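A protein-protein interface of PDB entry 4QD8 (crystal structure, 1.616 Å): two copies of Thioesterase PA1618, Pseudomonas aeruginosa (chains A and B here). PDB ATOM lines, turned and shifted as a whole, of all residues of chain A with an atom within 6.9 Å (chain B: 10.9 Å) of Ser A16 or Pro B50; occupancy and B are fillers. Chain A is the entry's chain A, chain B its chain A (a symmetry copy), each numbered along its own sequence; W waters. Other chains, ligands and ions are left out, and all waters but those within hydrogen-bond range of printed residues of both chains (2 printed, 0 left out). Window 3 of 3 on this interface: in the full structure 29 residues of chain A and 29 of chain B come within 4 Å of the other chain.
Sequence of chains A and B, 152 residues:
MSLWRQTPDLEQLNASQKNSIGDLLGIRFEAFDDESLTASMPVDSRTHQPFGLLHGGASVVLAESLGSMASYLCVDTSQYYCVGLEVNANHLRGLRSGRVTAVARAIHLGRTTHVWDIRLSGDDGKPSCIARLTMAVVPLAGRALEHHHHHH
The guanidinium group (NH2) of Arg B46 lies within salt-bridge range of the side-chain carboxylate (OD2) of Asp B44. O of Thr B47 sits at hydrogen-bond distance from N of His B55, 2.9 Å away. A ring nitrogen (NE2) of His B48 lies within hydrogen-bond range of the backbone carbonyl oxygen of Arg B96 (2.8 Å). N of Phe B51 is in hydrogen-bond range of OE1 of Gln B49 (2.8 Å). OE1 of Gln B49 sits at hydrogen-bond distance from N of Gly B52, at 3.1 Å. ND1 of His B55 is in hydrogen-bond range of N of Gly B57 (2.9 Å).
No position is printed for both chains.
Of the 17 printed residues of chain A, 5 touch a printed residue of chain B. Hydrophobic or aromatic side chains of chain A within 4 Å of the printed part of chain B: Ile A21. Hydrophobic or aromatic side chains of chain B that line the printed part of chain A: Pro B50, His B55 and Ala B58. Among the printed residues, 11 pairs touch across the chains. Among the printed residues, no Asp or Glu carboxylate lies within 4 Å of a Lys or Arg side-chain nitrogen of the other chain.
Ser A16 touches Pro B50. Ser A20 touches Ser B45 (CA to O, 3.3 Å). O of His B48 touches CB of Ser A20 (3.2 Å). Ser A20 touches Gln B49. Ile A21 touches Ser B45. Arg B46 touches Ile A21 (O to CB, 3.2 Å). CD2 of His B55 touches CG2 of Ile A21, at 3.2 Å. Ala B58 touches Ile A21.
No residue of chain B comes within 4 Å of Ala A15. Gln A17 touches none of the printed residues of chain B. Of the printed residues of chain B, Asn A19 touches Ser B45. Printed residues of chain B within 4 Å of Ile A21: Ser B45, Arg B46, His B48, His B55 and Ala B58. Of the printed residues of chain B, Ser A65 touches His B55 (2.8 Å). Of the printed residues of chain A, Arg B46 touches Ile A21. Printed residues of chain A within 4 Å of Pro B50: Ser A16 (3.5 Å). Leu B53 touches none of the printed residues of chain A. Printed residues of chain A within 4 Å of Ala B58: Ile A21. Leu B95 touches none of the printed residues of chain A. The nearest printed residue of chain A that does not touch His B48 is Asn A19 (4.5 Å).
O of His B48 sits at hydrogen-bond distance from N of Ile A21 (2.9 Å). OG of Ser A65 sits at hydrogen-bond distance from NE2 of His B55 (2.8 Å). O of Asn A19 lies close to O of Ser B45 (3.5 Å).
Water W1 lies within hydrogen-bond range of O of Asn A19 (2.8 Å) and ND1 of His B48 (2.8 Å). Water W2 lies within hydrogen-bond range of O of Ser B45 (3.1 Å) and O of Ser A20 (3.4 Å).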
ATOM      1  N   LEU A  10     -12.026 -28.363   7.039  1.00  0.00           N
ATOM      2  CA  LEU A  10     -10.945 -27.480   7.481  1.00  0.00           C
ATOM      3  C   LEU A  10      -9.807 -27.409   6.468  1.00  0.00           C
ATOM      4  O   LEU A  10      -9.204 -26.354   6.277  1.00  0.00           O
ATOM      5  CB  LEU A  10     -10.445 -27.912   8.861  1.00  0.00           C
ATOM      6  CG  LEU A  10     -11.481 -27.887   9.988  1.00  0.00           C
ATOM      7  CD1 LEU A  10     -10.947 -28.472  11.275  1.00  0.00           C
ATOM      8  CD2 LEU A  10     -11.986 -26.482  10.247  1.00  0.00           C
ATOM      9  N   GLU A  11      -9.529 -28.519   5.786  1.00  0.00           N
ATOM     10  CA  GLU A  11      -8.458 -28.529   4.797  1.00  0.00           C
ATOM     11  C   GLU A  11      -8.751 -27.576   3.647  1.00  0.00           C
ATOM     12  O   GLU A  11      -7.879 -26.817   3.228  1.00  0.00           O
ATOM     13  CB  GLU A  11      -8.229 -29.942   4.240  1.00  0.00           C
ATOM     14  CG  GLU A  11      -6.888 -30.095   3.532  1.00  0.00           C
ATOM     15  CD  GLU A  11      -5.748 -30.240   4.518  1.00  0.00           C
ATOM     16  OE1 GLU A  11      -4.580 -30.005   4.141  1.00  0.00           O
ATOM     17  OE2 GLU A  11      -6.018 -30.598   5.676  1.00  0.00           O
ATOM     18  N   GLN A  12      -9.982 -27.623   3.144  1.00  0.00           N
ATOM     19  CA  GLN A  12     -10.399 -26.764   2.045  1.00  0.00           C
ATOM     20  C   GLN A  12     -10.391 -25.310   2.489  1.00  0.00           C
ATOM     21  O   GLN A  12      -9.953 -24.422   1.744  1.00  0.00           O
ATOM     22  CB  GLN A  12     -11.812 -27.136   1.579  1.00  0.00           C
ATOM     23  CG  GLN A  12     -11.951 -28.482   0.889  1.00  0.00           C
ATOM     24  CD  GLN A  12     -13.409 -28.843   0.643  1.00  0.00           C
ATOM     25  OE1 GLN A  12     -14.263 -28.641   1.508  1.00  0.00           O
ATOM     26  NE2 GLN A  12     -13.701 -29.367  -0.543  1.00  0.00           N
ATOM     27  N   LEU A  13     -10.891 -25.060   3.695  1.00  0.00           N
ATOM     28  CA  LEU A  13     -10.926 -23.692   4.214  1.00  0.00           C
ATOM     29  C   LEU A  13      -9.506 -23.142   4.259  1.00  0.00           C
ATOM     30  O   LEU A  13      -9.233 -22.036   3.777  1.00  0.00           O
ATOM     31  CB  LEU A  13     -11.578 -23.622   5.601  1.00  0.00           C
ATOM     32  CG  LEU A  13     -13.018 -24.148   5.722  1.00  0.00           C
ATOM     33  CD1 LEU A  13     -13.552 -23.904   7.118  1.00  0.00           C
ATOM     34  CD2 LEU A  13     -13.911 -23.496   4.698  1.00  0.00           C
ATOM     35  N   ASN A  14      -8.593 -23.925   4.822  1.00  0.00           N
ATOM     36  CA  ASN A  14      -7.198 -23.512   4.877  1.00  0.00           C
ATOM     37  C   ASN A  14      -6.555 -23.405   3.508  1.00  0.00           C
ATOM     38  O   ASN A  14      -5.903 -22.413   3.200  1.00  0.00           O
ATOM     39  CB  ASN A  14      -6.393 -24.439   5.785  1.00  0.00           C
ATOM     40  CG  ASN A  14      -6.697 -24.208   7.251  1.00  0.00           C
ATOM     41  OD1 ASN A  14      -6.827 -23.064   7.685  1.00  0.00           O
ATOM     42  ND2 ASN A  14      -6.839 -25.280   8.015  1.00  0.00           N
ATOM     43  N   ALA A  15      -6.737 -24.432   2.681  1.00  0.00           N
ATOM     44  CA  ALA A  15      -6.191 -24.409   1.332  1.00  0.00           C
ATOM     45  C   ALA A  15      -6.690 -23.207   0.516  1.00  0.00           C
ATOM     46  O   ALA A  15      -5.957 -22.660  -0.304  1.00  0.00           O
ATOM     47  CB  ALA A  15      -6.496 -25.728   0.603  1.00  0.00           C
ATOM     48  N   SER A  16      -7.934 -22.792   0.754  1.00  0.00           N
ATOM     49  CA  SER A  16      -8.529 -21.721  -0.049  1.00  0.00           C
ATOM     50  C   SER A  16      -7.872 -20.366   0.188  1.00  0.00           C
ATOM     51  O   SER A  16      -8.044 -19.441  -0.606  1.00  0.00           O
ATOM     52  CB  SER A  16     -10.045 -21.640   0.173  1.00  0.00           C
ATOM     53  OG  SER A  16     -10.361 -21.190   1.478  1.00  0.00           O
ATOM     54  N   GLN A  17      -7.089 -20.251   1.261  1.00  0.00           N
ATOM     55  CA  GLN A  17      -6.456 -18.981   1.608  1.00  0.00           C
ATOM     56  C   GLN A  17      -5.166 -18.706   0.861  1.00  0.00           C
ATOM     57  O   GLN A  17      -4.550 -17.658   1.049  1.00  0.00           O
ATOM     58  CB  GLN A  17      -6.146 -18.933   3.101  1.00  0.00           C
ATOM     59  CG  GLN A  17      -7.338 -18.999   3.990  1.00  0.00           C
ATOM     60  CD  GLN A  17      -6.953 -18.755   5.421  1.00  0.00           C
ATOM     61  OE1 GLN A  17      -7.389 -17.777   6.033  1.00  0.00           O
ATOM     62  NE2 GLN A  17      -6.117 -19.633   5.968  1.00  0.00           N
ATOM     63  N   LYS A  18      -4.736 -19.656   0.036  1.00  0.00           N
ATOM     64  CA  LYS A  18      -3.491 -19.504  -0.697  1.00  0.00           C
ATOM     65  C   LYS A  18      -3.495 -18.203  -1.494  1.00  0.00           C
ATOM     66  O   LYS A  18      -4.510 -17.845  -2.089  1.00  0.00           O
ATOM     67  CB  LYS A  18      -3.291 -20.698  -1.630  1.00  0.00           C
ATOM     68  CG  LYS A  18      -1.969 -20.709  -2.365  1.00  0.00           C
ATOM     69  CD  LYS A  18      -2.013 -21.755  -3.469  1.00  0.00           C
ATOM     70  CE  LYS A  18      -0.655 -21.941  -4.114  1.00  0.00           C
ATOM     71  NZ  LYS A  18      -0.740 -22.922  -5.228  1.00  0.00           N
ATOM     72  N   ASN A  19      -2.370 -17.490  -1.468  1.00  0.00           N
ATOM     73  CA  ASN A  19      -2.231 -16.198  -2.145  1.00  0.00           C
ATOM     74  C   ASN A  19      -3.202 -15.133  -1.658  1.00  0.00           C
ATOM     75  O   ASN A  19      -3.645 -14.286  -2.438  1.00  0.00           O
ATOM     76  CB  ASN A  19      -2.373 -16.341  -3.665  1.00  0.00           C
ATOM     77  CG  ASN A  19      -1.344 -17.269  -4.268  1.00  0.00           C
ATOM     78  OD1 ASN A  19      -0.225 -17.390  -3.769  1.00  0.00           O
ATOM     79  ND2 ASN A  19      -1.720 -17.933  -5.360  1.00  0.00           N
ATOM     80  N   SER A  20      -3.537 -15.165  -0.373  1.00  0.00           N
ATOM     81  CA  SER A  20      -4.372 -14.118   0.199  1.00  0.00           C
ATOM     82  C   SER A  20      -3.818 -13.772   1.582  1.00  0.00           C
ATOM     83  O   SER A  20      -2.892 -14.424   2.062  1.00  0.00           O
ATOM     84  CB  SER A  20      -5.832 -14.562   0.290  1.00  0.00           C
ATOM     85  OG  SER A  20      -6.008 -15.496   1.334  1.00  0.00           O
ATOM     86  N   ILE A  21      -4.375 -12.752   2.228  1.00  0.00           N
ATOM     87  CA  ILE A  21      -3.783 -12.285   3.485  1.00  0.00           C
ATOM     88  C   ILE A  21      -3.818 -13.343   4.587  1.00  0.00           C
ATOM     89  O   ILE A  21      -2.915 -13.404   5.443  1.00  0.00           O
ATOM     90  CB  ILE A  21      -4.440 -10.957   3.949  1.00  0.00           C
ATOM     91  CG1 ILE A  21      -3.650 -10.323   5.109  1.00  0.00           C
ATOM     92  CG2 ILE A  21      -5.908 -11.170   4.296  1.00  0.00           C
ATOM     93  CD1 ILE A  21      -4.120  -8.921   5.453  1.00  0.00           C
ATOM     94  N   GLY A  22      -4.845 -14.186   4.583  1.00  0.00           N
ATOM     95  CA  GLY A  22      -4.968 -15.202   5.617  1.00  0.00           C
ATOM     96  C   GLY A  22      -3.787 -16.160   5.631  1.00  0.00           C
ATOM     97  O   GLY A  22      -3.303 -16.568   6.695  1.00  0.00           O
ATOM     98  N   PHE A  29      -7.826 -22.300  10.171  1.00  0.00           N
ATOM     99  CA  PHE A  29      -9.126 -22.800  10.609  1.00  0.00           C
ATOM    100  C   PHE A  29      -8.901 -24.099  11.365  1.00  0.00           C
ATOM    101  O   PHE A  29      -8.268 -25.015  10.833  1.00  0.00           O
ATOM    102  CB  PHE A  29     -10.059 -22.994   9.413  1.00  0.00           C
ATOM    103  CG  PHE A  29     -10.468 -21.693   8.783  1.00  0.00           C
ATOM    104  CD1 PHE A  29      -9.650 -21.072   7.855  1.00  0.00           C
ATOM    105  CD2 PHE A  29     -11.646 -21.066   9.165  1.00  0.00           C
ATOM    106  CE1 PHE A  29     -10.006 -19.844   7.297  1.00  0.00           C
ATOM    107  CE2 PHE A  29     -12.012 -19.853   8.619  1.00  0.00           C
ATOM    108  CZ  PHE A  29     -11.188 -19.234   7.681  1.00  0.00           C
ATOM    109  N   SER A  65     -11.961 -12.748   8.378  1.00  0.00           N
ATOM    110  CA  SER A  65     -11.684 -13.995   7.658  1.00  0.00           C
ATOM    111  C   SER A  65     -12.628 -15.081   8.135  1.00  0.00           C
ATOM    112  O   SER A  65     -13.207 -15.810   7.333  1.00  0.00           O
ATOM    113  CB  SER A  65     -10.248 -14.486   7.909  1.00  0.00           C
ATOM    114  OG  SER A  65      -9.346 -13.943   6.968  1.00  0.00           O
ATOM    115  N   SER A  68     -16.426 -14.221   7.368  1.00  0.00           N
ATOM    116  CA  SER A  68     -16.721 -14.286   5.936  1.00  0.00           C
ATOM    117  C   SER A  68     -16.780 -15.734   5.468  1.00  0.00           C
ATOM    118  O   SER A  68     -17.636 -16.099   4.652  1.00  0.00           O
ATOM    119  CB  SER A  68     -15.690 -13.512   5.123  1.00  0.00           C
ATOM    120  OG  SER A  68     -15.726 -12.140   5.485  1.00  0.00           O
ATOM    121  N   MET A  69     -15.883 -16.558   5.993  1.00  0.00           N
ATOM    122  CA  MET A  69     -15.877 -17.976   5.644  1.00  0.00           C
ATOM    123  C   MET A  69     -17.130 -18.642   6.197  1.00  0.00           C
ATOM    124  O   MET A  69     -17.767 -19.461   5.523  1.00  0.00           O
ATOM    125  CB  MET A  69     -14.633 -18.671   6.188  1.00  0.00           C
ATOM    126  CG  MET A  69     -14.469 -20.090   5.681  1.00  0.00           C
ATOM    127  SD  MET A  69     -14.093 -20.081   3.919  1.00  0.00           S
ATOM    128  CE  MET A  69     -12.393 -19.508   3.947  1.00  0.00           C
ATOM    129  N   ASP B  44      -3.244  -6.334  -3.392  1.00  0.00           N
ATOM    130  CA  ASP B  44      -2.630  -7.449  -4.103  1.00  0.00           C
ATOM    131  C   ASP B  44      -2.733  -8.728  -3.274  1.00  0.00           C
ATOM    132  O   ASP B  44      -3.539  -8.795  -2.355  1.00  0.00           O
ATOM    133  CB  ASP B  44      -1.187  -7.115  -4.556  1.00  0.00           C
ATOM    134  CG  ASP B  44      -0.223  -6.866  -3.397  1.00  0.00           C
ATOM    135  OD1 ASP B  44      -0.423  -7.386  -2.281  1.00  0.00           O
ATOM    136  OD2 ASP B  44       0.772  -6.156  -3.626  1.00  0.00           O
ATOM    137  N   SER B  45      -1.943  -9.750  -3.598  1.00  0.00           N
ATOM    138  CA  SER B  45      -2.035 -11.023  -2.881  1.00  0.00           C
ATOM    139  C   SER B  45      -1.763 -10.907  -1.379  1.00  0.00           C
ATOM    140  O   SER B  45      -2.222 -11.738  -0.593  1.00  0.00           O
ATOM    141  CB  SER B  45      -1.109 -12.071  -3.512  1.00  0.00           C
ATOM    142  OG  SER B  45       0.224 -11.614  -3.514  1.00  0.00           O
ATOM    143  N   ARG B  46      -1.037  -9.871  -0.976  1.00  0.00           N
ATOM    144  CA  ARG B  46      -0.740  -9.689   0.442  1.00  0.00           C
ATOM    145  C   ARG B  46      -1.977  -9.252   1.225  1.00  0.00           C
ATOM    146  O   ARG B  46      -2.074  -9.498   2.425  1.00  0.00           O
ATOM    147  CB  ARG B  46       0.367  -8.651   0.626  1.00  0.00           C
ATOM    148  CG  ARG B  46       1.743  -9.107   0.175  1.00  0.00           C
ATOM    149  CD  ARG B  46       2.699  -7.930   0.116  1.00  0.00           C
ATOM    150  NE  ARG B  46       2.407  -7.045  -1.013  1.00  0.00           N
ATOM    151  CZ  ARG B  46       3.067  -5.925  -1.290  1.00  0.00           C
ATOM    152  NH1 ARG B  46       4.062  -5.524  -0.507  1.00  0.00           N
ATOM    153  NH2 ARG B  46       2.733  -5.196  -2.347  1.00  0.00           N
ATOM    154  N   THR B  47      -2.909  -8.595   0.539  1.00  0.00           N
ATOM    155  CA  THR B  47      -4.035  -7.932   1.201  1.00  0.00           C
ATOM    156  C   THR B  47      -5.381  -8.419   0.661  1.00  0.00           C
ATOM    157  O   THR B  47      -6.435  -8.011   1.146  1.00  0.00           O
ATOM    158  CB  THR B  47      -3.957  -6.394   1.048  1.00  0.00           C
ATOM    159  OG1 THR B  47      -3.864  -6.068  -0.340  1.00  0.00           O
ATOM    160  CG2 THR B  47      -2.729  -5.808   1.782  1.00  0.00           C
ATOM    161  N   HIS B  48      -5.360  -9.295  -0.344  1.00  0.00           N
ATOM    162  CA  HIS B  48      -6.603  -9.878  -0.854  1.00  0.00           C
ATOM    163  C   HIS B  48      -7.264 -10.852   0.125  1.00  0.00           C
ATOM    164  O   HIS B  48      -6.584 -11.492   0.937  1.00  0.00           O
ATOM    165  CB  HIS B  48      -6.323 -10.667  -2.148  1.00  0.00           C
ATOM    166  CG  HIS B  48      -6.286  -9.838  -3.391  1.00  0.00           C
ATOM    167  ND1 HIS B  48      -5.707 -10.297  -4.560  1.00  0.00           N
ATOM    168  CD2 HIS B  48      -6.759  -8.598  -3.667  1.00  0.00           C
ATOM    169  CE1 HIS B  48      -5.822  -9.372  -5.496  1.00  0.00           C
ATOM    170  NE2 HIS B  48      -6.447  -8.330  -4.980  1.00  0.00           N
ATOM    171  N   GLN B  49      -8.591 -10.981   0.044  1.00  0.00           N
ATOM    172  CA  GLN B  49      -9.276 -12.155   0.603  1.00  0.00           C
ATOM    173  C   GLN B  49      -9.331 -13.231  -0.504  1.00  0.00           C
ATOM    174  O   GLN B  49      -8.837 -12.981  -1.601  1.00  0.00           O
ATOM    175  CB  GLN B  49     -10.655 -11.783   1.189  1.00  0.00           C
ATOM    176  CG  GLN B  49     -11.461 -10.743   0.428  1.00  0.00           C
ATOM    177  CD  GLN B  49     -12.235 -11.357  -0.711  1.00  0.00           C
ATOM    178  OE1 GLN B  49     -11.654 -11.779  -1.709  1.00  0.00           O
ATOM    179  NE2 GLN B  49     -13.549 -11.425  -0.563  1.00  0.00           N
ATOM    180  N   PRO B  50      -9.886 -14.431  -0.216  1.00  0.00           N
ATOM    181  CA  PRO B  50      -9.696 -15.507  -1.209  1.00  0.00           C
ATOM    182  C   PRO B  50     -10.358 -15.310  -2.575  1.00  0.00           C
ATOM    183  O   PRO B  50     -10.028 -16.052  -3.508  1.00  0.00           O
ATOM    184  CB  PRO B  50     -10.272 -16.732  -0.496  1.00  0.00           C
ATOM    185  CG  PRO B  50     -10.022 -16.446   0.960  1.00  0.00           C
ATOM    186  CD  PRO B  50     -10.319 -14.977   1.082  1.00  0.00           C
ATOM    187  N   PHE B  51     -11.238 -14.323  -2.714  1.00  0.00           N
ATOM    188  CA  PHE B  51     -11.930 -14.115  -3.985  1.00  0.00           C
ATOM    189  C   PHE B  51     -11.348 -12.973  -4.785  1.00  0.00           C
ATOM    190  O   PHE B  51     -11.910 -12.558  -5.790  1.00  0.00           O
ATOM    191  CB  PHE B  51     -13.422 -13.914  -3.745  1.00  0.00           C
ATOM    192  CG  PHE B  51     -14.050 -15.056  -3.029  1.00  0.00           C
ATOM    193  CD1 PHE B  51     -14.499 -16.159  -3.734  1.00  0.00           C
ATOM    194  CD2 PHE B  51     -14.140 -15.058  -1.647  1.00  0.00           C
ATOM    195  CE1 PHE B  51     -15.058 -17.236  -3.080  1.00  0.00           C
ATOM    196  CE2 PHE B  51     -14.693 -16.132  -0.980  1.00  0.00           C
ATOM    197  CZ  PHE B  51     -15.157 -17.225  -1.700  1.00  0.00           C
ATOM    198  N   GLY B  52     -10.210 -12.466  -4.336  1.00  0.00           N
ATOM    199  CA  GLY B  52      -9.473 -11.493  -5.102  1.00  0.00           C
ATOM    200  C   GLY B  52      -9.851 -10.043  -4.854  1.00  0.00           C
ATOM    201  O   GLY B  52      -9.402  -9.167  -5.587  1.00  0.00           O
ATOM    202  N   LEU B  53     -10.672  -9.793  -3.830  1.00  0.00           N
ATOM    203  CA  LEU B  53     -11.017  -8.430  -3.417  1.00  0.00           C
ATOM    204  C   LEU B  53     -10.138  -8.060  -2.234  1.00  0.00           C
ATOM    205  O   LEU B  53      -9.693  -8.932  -1.492  1.00  0.00           O
ATOM    206  CB  LEU B  53     -12.467  -8.357  -2.942  1.00  0.00           C
ATOM    207  CG  LEU B  53     -13.609  -8.620  -3.913  1.00  0.00           C
ATOM    208  CD1 LEU B  53     -14.917  -8.762  -3.153  1.00  0.00           C
ATOM    209  CD2 LEU B  53     -13.685  -7.455  -4.868  1.00  0.00           C
ATOM    210  N   LEU B  54      -9.893  -6.769  -2.043  1.00  0.00           N
ATOM    211  CA  LEU B  54      -9.231  -6.321  -0.820  1.00  0.00           C
ATOM    212  C   LEU B  54      -9.998  -6.840   0.407  1.00  0.00           C
ATOM    213  O   LEU B  54     -11.200  -6.634   0.532  1.00  0.00           O
ATOM    214  CB  LEU B  54      -9.164  -4.785  -0.816  1.00  0.00           C
ATOM    215  CG  LEU B  54      -8.648  -4.145   0.468  1.00  0.00           C
ATOM    216  CD1 LEU B  54      -7.215  -4.607   0.723  1.00  0.00           C
ATOM    217  CD2 LEU B  54      -8.744  -2.638   0.306  1.00  0.00           C
ATOM    218  N   HIS B  55      -9.295  -7.539   1.300  1.00  0.00           N
ATOM    219  CA  HIS B  55      -9.874  -8.085   2.535  1.00  0.00           C
ATOM    220  C   HIS B  55     -10.315  -6.918   3.413  1.00  0.00           C
ATOM    221  O   HIS B  55      -9.554  -5.984   3.613  1.00  0.00           O
ATOM    222  CB  HIS B  55      -8.785  -8.910   3.252  1.00  0.00           C
ATOM    223  CG  HIS B  55      -9.264  -9.775   4.374  1.00  0.00           C
ATOM    224  ND1 HIS B  55      -9.858  -9.282   5.521  1.00  0.00           N
ATOM    225  CD2 HIS B  55      -9.143 -11.112   4.572  1.00  0.00           C
ATOM    226  CE1 HIS B  55     -10.105 -10.272   6.352  1.00  0.00           C
ATOM    227  NE2 HIS B  55      -9.677 -11.397   5.806  1.00  0.00           N
ATOM    228  N   GLY B  56     -11.547  -6.965   3.917  1.00  0.00           N
ATOM    229  CA  GLY B  56     -12.066  -5.872   4.722  1.00  0.00           C
ATOM    230  C   GLY B  56     -11.249  -5.660   5.979  1.00  0.00           C
ATOM    231  O   GLY B  56     -11.111  -4.537   6.464  1.00  0.00           O
ATOM    232  N   GLY B  57     -10.679  -6.731   6.504  1.00  0.00           N
ATOM    233  CA  GLY B  57      -9.776  -6.591   7.639  1.00  0.00           C
ATOM    234  C   GLY B  57      -8.501  -5.847   7.289  1.00  0.00           C
ATOM    235  O   GLY B  57      -7.939  -5.122   8.117  1.00  0.00           O
ATOM    236  N   ALA B  58      -8.018  -6.025   6.066  1.00  0.00           N
ATOM    237  CA  ALA B  58      -6.822  -5.307   5.624  1.00  0.00           C
ATOM    238  C   ALA B  58      -7.090  -3.798   5.586  1.00  0.00           C
ATOM    239  O   ALA B  58      -6.209  -2.994   5.932  1.00  0.00           O
ATOM    240  CB  ALA B  58      -6.349  -5.827   4.260  1.00  0.00           C
ATOM    241  N   LEU B  95     -12.435  -3.414  -3.891  1.00  0.00           N
ATOM    242  CA  LEU B  95     -11.260  -3.069  -4.696  1.00  0.00           C
ATOM    243  C   LEU B  95     -10.532  -4.350  -5.068  1.00  0.00           C
ATOM    244  O   LEU B  95     -10.480  -5.283  -4.268  1.00  0.00           O
ATOM    245  CB  LEU B  95     -10.300  -2.154  -3.931  1.00  0.00           C
ATOM    246  CG  LEU B  95     -10.850  -0.788  -3.529  1.00  0.00           C
ATOM    247  CD1 LEU B  95      -9.869  -0.091  -2.598  1.00  0.00           C
ATOM    248  CD2 LEU B  95     -11.099   0.030  -4.768  1.00  0.00           C
ATOM    249  N   ARG B  96      -9.966  -4.396  -6.275  1.00  0.00           N
ATOM    250  CA  ARG B  96      -9.260  -5.596  -6.743  1.00  0.00           C
ATOM    251  C   ARG B  96      -7.768  -5.372  -7.001  1.00  0.00           C
ATOM    252  O   ARG B  96      -6.970  -6.292  -6.878  1.00  0.00           O
ATOM    253  CB  ARG B  96      -9.921  -6.167  -8.006  1.00  0.00           C
ATOM    254  CG  ARG B  96     -11.251  -6.850  -7.760  1.00  0.00           C
ATOM    255  CD  ARG B  96     -11.674  -7.729  -8.944  1.00  0.00           C
ATOM    256  NE  ARG B  96     -12.949  -8.406  -8.698  1.00  0.00           N
ATOM    257  CZ  ARG B  96     -13.065  -9.611  -8.146  1.00  0.00           C
ATOM    258  NH1 ARG B  96     -11.981 -10.284  -7.776  1.00  0.00           N
ATOM    259  NH2 ARG B  96     -14.267 -10.148  -7.960  1.00  0.00           N
HETATM  260  O   HOH W   1      -4.874 -13.006  -4.590  1.00  0.00           O
HETATM  261  O   HOH W   2      -0.065 -13.786   0.210  1.00  0.00           O
